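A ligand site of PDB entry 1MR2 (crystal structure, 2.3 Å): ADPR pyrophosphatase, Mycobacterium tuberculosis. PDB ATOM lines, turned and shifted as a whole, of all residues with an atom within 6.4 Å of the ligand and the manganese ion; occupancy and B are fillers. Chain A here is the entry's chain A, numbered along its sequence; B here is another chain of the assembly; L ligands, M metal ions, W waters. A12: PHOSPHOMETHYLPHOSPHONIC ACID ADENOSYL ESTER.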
ATOM      1  N   ALA A  18      -0.171 -22.665 -35.134  1.00  0.00           N
ATOM      2  CA  ALA A  18       0.092 -22.816 -33.715  1.00  0.00           C
ATOM      3  C   ALA A  18       0.365 -24.275 -33.346  1.00  0.00           C
ATOM      4  O   ALA A  18       1.315 -24.555 -32.617  1.00  0.00           O
ATOM      5  CB  ALA A  18      -1.098 -22.297 -32.928  1.00  0.00           C
ATOM      6  N   ILE A  19      -0.449 -25.204 -33.842  1.00  0.00           N
ATOM      7  CA  ILE A  19      -0.268 -26.613 -33.534  1.00  0.00           C
ATOM      8  C   ILE A  19       0.030 -27.532 -34.720  1.00  0.00           C
ATOM      9  O   ILE A  19       0.270 -28.733 -34.539  1.00  0.00           O
ATOM     10  CB  ILE A  19      -1.481 -27.206 -32.764  1.00  0.00           C
ATOM     11  CG1 ILE A  19      -2.743 -27.135 -33.615  1.00  0.00           C
ATOM     12  CG2 ILE A  19      -1.678 -26.456 -31.458  1.00  0.00           C
ATOM     13  CD1 ILE A  19      -3.857 -28.023 -33.091  1.00  0.00           C
ATOM     14  N   PHE A  20       0.016 -26.979 -35.930  1.00  0.00           N
ATOM     15  CA  PHE A  20       0.332 -27.760 -37.125  1.00  0.00           C
ATOM     16  C   PHE A  20       0.852 -26.878 -38.248  1.00  0.00           C
ATOM     17  O   PHE A  20       0.744 -25.660 -38.192  1.00  0.00           O
ATOM     18  CB  PHE A  20      -0.887 -28.564 -37.599  1.00  0.00           C
ATOM     19  CG  PHE A  20      -2.094 -27.730 -37.966  1.00  0.00           C
ATOM     20  CD1 PHE A  20      -2.104 -26.927 -39.100  1.00  0.00           C
ATOM     21  CD2 PHE A  20      -3.243 -27.783 -37.174  1.00  0.00           C
ATOM     22  CE1 PHE A  20      -3.233 -26.194 -39.455  1.00  0.00           C
ATOM     23  CE2 PHE A  20      -4.384 -27.057 -37.516  1.00  0.00           C
ATOM     24  CZ  PHE A  20      -4.381 -26.256 -38.656  1.00  0.00           C
ATOM     25  N   ALA A  45      -0.169 -36.831 -30.384  1.00  0.00           N
ATOM     26  CA  ALA A  45      -0.824 -36.696 -29.094  1.00  0.00           C
ATOM     27  C   ALA A  45      -0.836 -38.020 -28.337  1.00  0.00           C
ATOM     28  O   ALA A  45      -0.467 -39.063 -28.885  1.00  0.00           O
ATOM     29  CB  ALA A  45      -2.247 -36.197 -29.291  1.00  0.00           C
ATOM     30  N   GLN A  62     -15.855 -32.290 -23.653  1.00  0.00           N
ATOM     31  CA  GLN A  62     -15.222 -31.073 -24.133  1.00  0.00           C
ATOM     32  C   GLN A  62     -15.779 -30.494 -25.430  1.00  0.00           C
ATOM     33  O   GLN A  62     -16.114 -31.225 -26.365  1.00  0.00           O
ATOM     34  CB  GLN A  62     -13.719 -31.312 -24.269  1.00  0.00           C
ATOM     35  CG  GLN A  62     -12.913 -30.138 -24.786  1.00  0.00           C
ATOM     36  CD  GLN A  62     -11.427 -30.330 -24.588  1.00  0.00           C
ATOM     37  OE1 GLN A  62     -10.924 -31.465 -24.658  1.00  0.00           O
ATOM     38  NE2 GLN A  62     -10.697 -29.239 -24.340  1.00  0.00           N
ATOM     39  N   ARG A  64     -15.781 -28.950 -28.954  1.00  0.00           N
ATOM     40  CA  ARG A  64     -14.924 -29.046 -30.131  1.00  0.00           C
ATOM     41  C   ARG A  64     -15.380 -28.055 -31.200  1.00  0.00           C
ATOM     42  O   ARG A  64     -16.369 -28.291 -31.893  1.00  0.00           O
ATOM     43  CB  ARG A  64     -14.926 -30.465 -30.689  1.00  0.00           C
ATOM     44  CG  ARG A  64     -14.124 -31.450 -29.858  1.00  0.00           C
ATOM     45  CD  ARG A  64     -12.692 -30.958 -29.684  1.00  0.00           C
ATOM     46  NE  ARG A  64     -11.871 -31.854 -28.892  1.00  0.00           N
ATOM     47  CZ  ARG A  64     -10.585 -31.645 -28.615  1.00  0.00           C
ATOM     48  NH1 ARG A  64      -9.969 -30.555 -29.056  1.00  0.00           N
ATOM     49  NH2 ARG A  64      -9.905 -32.532 -27.890  1.00  0.00           N
ATOM     50  N   THR A  66     -14.353 -27.463 -34.061  1.00  0.00           N
ATOM     51  CA  THR A  66     -14.451 -28.071 -35.384  1.00  0.00           C
ATOM     52  C   THR A  66     -15.861 -28.593 -35.670  1.00  0.00           C
ATOM     53  O   THR A  66     -16.284 -28.625 -36.818  1.00  0.00           O
ATOM     54  CB  THR A  66     -13.422 -29.213 -35.540  1.00  0.00           C
ATOM     55  OG1 THR A  66     -13.338 -29.960 -34.336  1.00  0.00           O
ATOM     56  CG2 THR A  66     -12.051 -28.655 -35.898  1.00  0.00           C
ATOM     57  N   GLU A  73     -14.726 -37.627 -24.710  1.00  0.00           N
ATOM     58  CA  GLU A  73     -13.388 -38.075 -25.058  1.00  0.00           C
ATOM     59  C   GLU A  73     -12.545 -38.595 -23.895  1.00  0.00           C
ATOM     60  O   GLU A  73     -12.887 -38.453 -22.730  1.00  0.00           O
ATOM     61  CB  GLU A  73     -12.615 -36.940 -25.717  1.00  0.00           C
ATOM     62  CG  GLU A  73     -13.487 -35.975 -26.488  1.00  0.00           C
ATOM     63  CD  GLU A  73     -12.697 -34.812 -27.017  1.00  0.00           C
ATOM     64  OE1 GLU A  73     -11.858 -34.278 -26.257  1.00  0.00           O
ATOM     65  OE2 GLU A  73     -12.911 -34.419 -28.181  1.00  0.00           O
ATOM     66  N   LEU A  74     -11.396 -39.175 -24.249  1.00  0.00           N
ATOM     67  CA  LEU A  74     -10.473 -39.679 -23.254  1.00  0.00           C
ATOM     68  C   LEU A  74      -9.566 -38.523 -22.870  1.00  0.00           C
ATOM     69  O   LEU A  74      -9.407 -37.576 -23.643  1.00  0.00           O
ATOM     70  CB  LEU A  74      -9.624 -40.817 -23.824  1.00  0.00           C
ATOM     71  CG  LEU A  74     -10.354 -42.062 -24.341  1.00  0.00           C
ATOM     72  CD1 LEU A  74      -9.357 -43.005 -25.029  1.00  0.00           C
ATOM     73  CD2 LEU A  74     -11.059 -42.754 -23.169  1.00  0.00           C
ATOM     74  N   PRO A  75      -8.986 -38.569 -21.665  1.00  0.00           N
ATOM     75  CA  PRO A  75      -8.089 -37.479 -21.280  1.00  0.00           C
ATOM     76  C   PRO A  75      -6.942 -37.541 -22.291  1.00  0.00           C
ATOM     77  O   PRO A  75      -6.377 -38.604 -22.535  1.00  0.00           O
ATOM     78  CB  PRO A  75      -7.654 -37.868 -19.869  1.00  0.00           C
ATOM     79  CG  PRO A  75      -8.846 -38.595 -19.346  1.00  0.00           C
ATOM     80  CD  PRO A  75      -9.260 -39.460 -20.519  1.00  0.00           C
ATOM     81  N   ALA A  76      -6.613 -36.409 -22.884  1.00  0.00           N
ATOM     82  CA  ALA A  76      -5.561 -36.393 -23.885  1.00  0.00           C
ATOM     83  C   ALA A  76      -4.839 -35.048 -24.003  1.00  0.00           C
ATOM     84  O   ALA A  76      -5.365 -33.988 -23.624  1.00  0.00           O
ATOM     85  CB  ALA A  76      -6.159 -36.793 -25.233  1.00  0.00           C
ATOM     86  N   GLY A  77      -3.619 -35.096 -24.530  1.00  0.00           N
ATOM     87  CA  GLY A  77      -2.836 -33.894 -24.704  1.00  0.00           C
ATOM     88  C   GLY A  77      -1.922 -33.979 -25.916  1.00  0.00           C
ATOM     89  O   GLY A  77      -1.614 -35.070 -26.394  1.00  0.00           O
ATOM     90  N   LEU A  78      -1.505 -32.811 -26.418  1.00  0.00           N
ATOM     91  CA  LEU A  78      -0.618 -32.731 -27.573  1.00  0.00           C
ATOM     92  C   LEU A  78       0.793 -32.983 -27.099  1.00  0.00           C
ATOM     93  O   LEU A  78       1.109 -32.749 -25.941  1.00  0.00           O
ATOM     94  CB  LEU A  78      -0.691 -31.338 -28.183  1.00  0.00           C
ATOM     95  CG  LEU A  78      -2.040 -30.852 -28.736  1.00  0.00           C
ATOM     96  CD1 LEU A  78      -2.004 -29.362 -28.979  1.00  0.00           C
ATOM     97  CD2 LEU A  78      -2.345 -31.599 -30.018  1.00  0.00           C
ATOM     98  N   ASP A  80       3.273 -31.300 -27.335  1.00  0.00           N
ATOM     99  CA  ASP A  80       3.888 -29.986 -27.516  1.00  0.00           C
ATOM    100  C   ASP A  80       5.059 -29.723 -26.584  1.00  0.00           C
ATOM    101  O   ASP A  80       5.697 -28.671 -26.682  1.00  0.00           O
ATOM    102  CB  ASP A  80       2.846 -28.864 -27.366  1.00  0.00           C
ATOM    103  CG  ASP A  80       2.132 -28.896 -26.027  1.00  0.00           C
ATOM    104  OD1 ASP A  80       2.779 -29.261 -25.027  1.00  0.00           O
ATOM    105  OD2 ASP A  80       0.932 -28.553 -25.971  1.00  0.00           O
ATOM    106  N   GLU A  93      -1.292 -35.271 -18.217  1.00  0.00           N
ATOM    107  CA  GLU A  93      -2.625 -34.957 -18.699  1.00  0.00           C
ATOM    108  C   GLU A  93      -3.665 -35.697 -17.883  1.00  0.00           C
ATOM    109  O   GLU A  93      -4.728 -35.155 -17.569  1.00  0.00           O
ATOM    110  CB  GLU A  93      -2.739 -35.344 -20.178  1.00  0.00           C
ATOM    111  CG  GLU A  93      -3.804 -34.568 -20.944  1.00  0.00           C
ATOM    112  CD  GLU A  93      -3.528 -33.064 -21.003  1.00  0.00           C
ATOM    113  OE1 GLU A  93      -2.466 -32.670 -21.525  1.00  0.00           O
ATOM    114  OE2 GLU A  93      -4.383 -32.282 -20.530  1.00  0.00           O
ATOM    115  N   GLU A  97      -6.295 -33.503 -16.080  1.00  0.00           N
ATOM    116  CA  GLU A  97      -7.623 -33.651 -16.634  1.00  0.00           C
ATOM    117  C   GLU A  97      -8.661 -34.277 -15.702  1.00  0.00           C
ATOM    118  O   GLU A  97      -9.798 -33.801 -15.606  1.00  0.00           O
ATOM    119  CB  GLU A  97      -7.538 -34.462 -17.921  1.00  0.00           C
ATOM    120  CG  GLU A  97      -8.693 -34.235 -18.882  1.00  0.00           C
ATOM    121  CD  GLU A  97      -8.705 -32.824 -19.452  1.00  0.00           C
ATOM    122  OE1 GLU A  97      -7.646 -32.392 -19.975  1.00  0.00           O
ATOM    123  OE2 GLU A  97      -9.766 -32.156 -19.375  1.00  0.00           O
ATOM    124  N   THR B  36      -7.775 -18.470 -30.545  1.00  0.00           N
ATOM    125  CA  THR B  36      -7.550 -18.752 -31.962  1.00  0.00           C
ATOM    126  C   THR B  36      -7.735 -20.243 -32.230  1.00  0.00           C
ATOM    127  O   THR B  36      -7.185 -21.095 -31.508  1.00  0.00           O
ATOM    128  CB  THR B  36      -6.141 -18.332 -32.428  1.00  0.00           C
ATOM    129  OG1 THR B  36      -6.046 -16.908 -32.408  1.00  0.00           O
ATOM    130  CG2 THR B  36      -5.857 -18.842 -33.843  1.00  0.00           C
ATOM    131  N   ARG B  37      -8.512 -20.555 -33.266  1.00  0.00           N
ATOM    132  CA  ARG B  37      -8.757 -21.931 -33.651  1.00  0.00           C
ATOM    133  C   ARG B  37      -8.624 -22.091 -35.151  1.00  0.00           C
ATOM    134  O   ARG B  37      -9.420 -21.555 -35.920  1.00  0.00           O
ATOM    135  CB  ARG B  37     -10.161 -22.354 -33.207  1.00  0.00           C
ATOM    136  CG  ARG B  37     -10.249 -22.709 -31.726  1.00  0.00           C
ATOM    137  CD  ARG B  37      -9.493 -23.996 -31.429  1.00  0.00           C
ATOM    138  NE  ARG B  37      -9.474 -24.318 -30.001  1.00  0.00           N
ATOM    139  CZ  ARG B  37      -8.679 -23.743 -29.094  1.00  0.00           C
ATOM    140  NH1 ARG B  37      -7.811 -22.796 -29.458  1.00  0.00           N
ATOM    141  NH2 ARG B  37      -8.742 -24.112 -27.823  1.00  0.00           N
ATOM    142  N   GLU B  38      -7.587 -22.813 -35.560  1.00  0.00           N
ATOM    143  CA  GLU B  38      -7.321 -23.065 -36.966  1.00  0.00           C
ATOM    144  C   GLU B  38      -7.968 -24.404 -37.294  1.00  0.00           C
ATOM    145  O   GLU B  38      -7.691 -25.409 -36.665  1.00  0.00           O
ATOM    146  CB  GLU B  38      -5.809 -23.107 -37.230  1.00  0.00           C
ATOM    147  CG  GLU B  38      -5.178 -21.730 -37.216  1.00  0.00           C
ATOM    148  CD  GLU B  38      -3.677 -21.748 -37.412  1.00  0.00           C
ATOM    149  OE1 GLU B  38      -3.201 -22.430 -38.335  1.00  0.00           O
ATOM    150  OE2 GLU B  38      -2.974 -21.053 -36.640  1.00  0.00           O
ATOM    151  N   VAL B  39      -8.866 -24.373 -38.280  1.00  0.00           N
ATOM    152  CA  VAL B  39      -9.611 -25.537 -38.704  1.00  0.00           C
ATOM    153  C   VAL B  39      -9.324 -25.984 -40.137  1.00  0.00           C
ATOM    154  O   VAL B  39      -9.193 -25.158 -41.045  1.00  0.00           O
ATOM    155  CB  VAL B  39     -11.140 -25.244 -38.591  1.00  0.00           C
ATOM    156  CG1 VAL B  39     -11.947 -26.437 -39.086  1.00  0.00           C
ATOM    157  CG2 VAL B  39     -11.496 -24.909 -37.152  1.00  0.00           C
ATOM    158  N   PRO B 115     -10.749 -34.339 -34.163  1.00  0.00           N
ATOM    159  CA  PRO B 115     -11.616 -33.267 -33.658  1.00  0.00           C
ATOM    160  C   PRO B 115     -10.842 -32.039 -33.226  1.00  0.00           C
ATOM    161  O   PRO B 115     -11.409 -30.949 -33.130  1.00  0.00           O
ATOM    162  CB  PRO B 115     -12.356 -33.948 -32.496  1.00  0.00           C
ATOM    163  CG  PRO B 115     -12.353 -35.421 -32.875  1.00  0.00           C
ATOM    164  CD  PRO B 115     -10.936 -35.580 -33.383  1.00  0.00           C
ATOM    165  N   GLY B 116      -9.560 -32.203 -32.970  1.00  0.00           N
ATOM    166  CA  GLY B 116      -8.733 -31.093 -32.539  1.00  0.00           C
ATOM    167  C   GLY B 116      -8.462 -30.013 -33.570  1.00  0.00           C
ATOM    168  O   GLY B 116      -8.302 -28.844 -33.198  1.00  0.00           O
ATOM    169  N   PHE B 117      -8.415 -30.349 -34.860  1.00  0.00           N
ATOM    170  CA  PHE B 117      -8.133 -29.336 -35.880  1.00  0.00           C
ATOM    171  C   PHE B 117      -8.812 -29.505 -37.239  1.00  0.00           C
ATOM    172  O   PHE B 117      -8.488 -28.777 -38.177  1.00  0.00           O
ATOM    173  CB  PHE B 117      -6.623 -29.258 -36.136  1.00  0.00           C
ATOM    174  CG  PHE B 117      -6.050 -30.502 -36.754  1.00  0.00           C
ATOM    175  CD1 PHE B 117      -5.716 -31.598 -35.975  1.00  0.00           C
ATOM    176  CD2 PHE B 117      -5.906 -30.595 -38.153  1.00  0.00           C
ATOM    177  CE1 PHE B 117      -5.237 -32.775 -36.564  1.00  0.00           C
ATOM    178  CE2 PHE B 117      -5.438 -31.769 -38.749  1.00  0.00           C
ATOM    179  CZ  PHE B 117      -5.107 -32.859 -37.962  1.00  0.00           C
ATOM    180  N   SER B 118      -9.738 -30.444 -37.368  1.00  0.00           N
ATOM    181  CA  SER B 118     -10.398 -30.648 -38.644  1.00  0.00           C
ATOM    182  C   SER B 118     -11.860 -30.981 -38.451  1.00  0.00           C
ATOM    183  O   SER B 118     -12.235 -31.529 -37.413  1.00  0.00           O
ATOM    184  CB  SER B 118      -9.705 -31.788 -39.408  1.00  0.00           C
ATOM    185  OG  SER B 118     -10.355 -32.079 -40.634  1.00  0.00           O
HETATM  186  PB  A12 L   1      -6.487 -31.252 -26.886  1.00  0.00           P
HETATM  187  O1B A12 L   1      -7.531 -30.872 -27.927  1.00  0.00           O
HETATM  188  O2B A12 L   1      -5.585 -32.445 -27.408  1.00  0.00           O
HETATM  189  O3B A12 L   1      -7.343 -31.725 -25.619  1.00  0.00           O
HETATM  190  PA  A12 L   1      -5.906 -28.512 -26.222  1.00  0.00           P
HETATM  191  O1A A12 L   1      -7.359 -27.904 -26.352  1.00  0.00           O
HETATM  192  O2A A12 L   1      -5.382 -28.812 -24.769  1.00  0.00           O
HETATM  193  C3A A12 L   1      -5.758 -29.885 -27.028  1.00  0.00           C
HETATM  194  O5' A12 L   1      -4.943 -27.344 -26.706  1.00  0.00           O
HETATM  195  C5' A12 L   1      -3.745 -26.847 -26.060  1.00  0.00           C
HETATM  196  C4' A12 L   1      -3.146 -25.677 -26.894  1.00  0.00           C
HETATM  197  O4' A12 L   1      -3.220 -25.782 -28.316  1.00  0.00           O
HETATM  198  C3' A12 L   1      -3.985 -24.452 -26.480  1.00  0.00           C
HETATM  199  O3' A12 L   1      -3.109 -23.484 -25.983  1.00  0.00           O
HETATM  200  C2' A12 L   1      -4.538 -23.878 -27.785  1.00  0.00           C
HETATM  201  O2' A12 L   1      -3.830 -22.866 -28.504  1.00  0.00           O
HETATM  202  C1' A12 L   1      -4.326 -25.025 -28.779  1.00  0.00           C
HETATM  203  N9  A12 L   1      -5.062 -25.420 -29.984  1.00  0.00           N
HETATM  204  C8  A12 L   1      -5.794 -26.587 -30.030  1.00  0.00           C
HETATM  205  N7  A12 L   1      -6.377 -26.700 -31.257  1.00  0.00           N
HETATM  206  C5  A12 L   1      -5.994 -25.590 -31.978  1.00  0.00           C
HETATM  207  C6  A12 L   1      -6.268 -25.181 -33.256  1.00  0.00           C
HETATM  208  N6  A12 L   1      -7.071 -25.970 -34.008  1.00  0.00           N
HETATM  209  N1  A12 L   1      -5.733 -23.983 -33.752  1.00  0.00           N
HETATM  210  C2  A12 L   1      -4.916 -23.152 -32.983  1.00  0.00           C
HETATM  211  N3  A12 L   1      -4.646 -23.589 -31.689  1.00  0.00           N
HETATM  212  C4  A12 L   1      -5.164 -24.771 -31.195  1.00  0.00           C
HETATM  213 MN    MN M   1      -6.709 -32.000 -23.559  1.00  0.00          MN
HETATM  214  O   HOH W   1      -7.854 -33.955 -21.819  1.00  0.00           O
HETATM  215  O   HOH W   2      -5.571 -34.297 -29.090  1.00  0.00           O
HETATM  216  O   HOH W   3      -9.050 -27.186 -30.001  1.00  0.00           O
HETATM  217  O   HOH W   4      -2.855 -30.232 -25.075  1.00  0.00           O
HETATM  218  O   HOH W   5      -6.025 -30.103 -30.686  1.00  0.00           O
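An oxygen (O1B) of the ligand lies within salt-bridge range of the guanidinium group of Arg 64, at 2.7 Å.
N of Glu 38 of chain B sits at hydrogen-bond distance from N1 of the ligand (2.8 Å).
O of Glu 38 of chain B lies within hydrogen-bond range of N6 of the ligand, 2.8 Å away.
The backbone carbonyl oxygen (O) of Gly 116 of chain B lies within hydrogen-bond range of a nitrogen (N6) of the ligand, 3.2 Å away.
Glu 93 touches the manganese ion.
OE1 of Glu 97 touches the manganese ion (3.7 Å).
Of the 24 residues printed, 3 come within 4 Å of the manganese ion.
The nearest printed residue that does not touch the manganese ion is Gln 62 (4.4 Å).
Water W1 lies within hydrogen-bond range of the side-chain carboxylate of Glu 97 and the backbone NH of Ala 76.
Water W4 lies within hydrogen-bond range of O2A of the ligand (2.9 Å) and N of Leu 78 (3.2 Å).
Water W3 lies within hydrogen-bond range of the guanidinium group of Arg 37 of chain B (2.9 Å) and a nitrogen (N7) of the ligand (3.0 Å).
The manganese ion is bound by O3B of the ligand (2.2 Å) and O of Ala 76 (2.4 Å).
The manganese ion has two donor atoms within binding distance.
Slightly farther from the manganese ion lies water W1 (2.9 Å).
The side-chain carboxylate (OE2) of Glu 73 lies within salt-bridge range of the guanidinium group (NE) of Arg 64 (2.9 Å).
The side-chain amide oxygen of Gln 62 sits close to the side-chain carboxylate of Glu 73 (3.4 Å).
Residues that only touch the ligand: Ile 19 (3.4 Å), Thr 36 of chain B (3.4 Å), Arg 37 of chain B (3.7 Å), Gln 62 (3.7 Å), Leu 78 (3.8 Å), Ala 18 (3.9 Å) and Phe 117 of chain B (3.9 Å).
Hydrophobic or aromatic side chains that line the ligand: Ala 18, Ile 19, Leu 78 and Phe 117 of chain B.
Of the 24 residues printed, 11 come within 4 Å of the ligand.
Along chain A the residues within 4 Å of the ligand span positions 18 to 78.
The nearest printed residue that does not touch the ligand is Gly 77 (4.1 Å).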
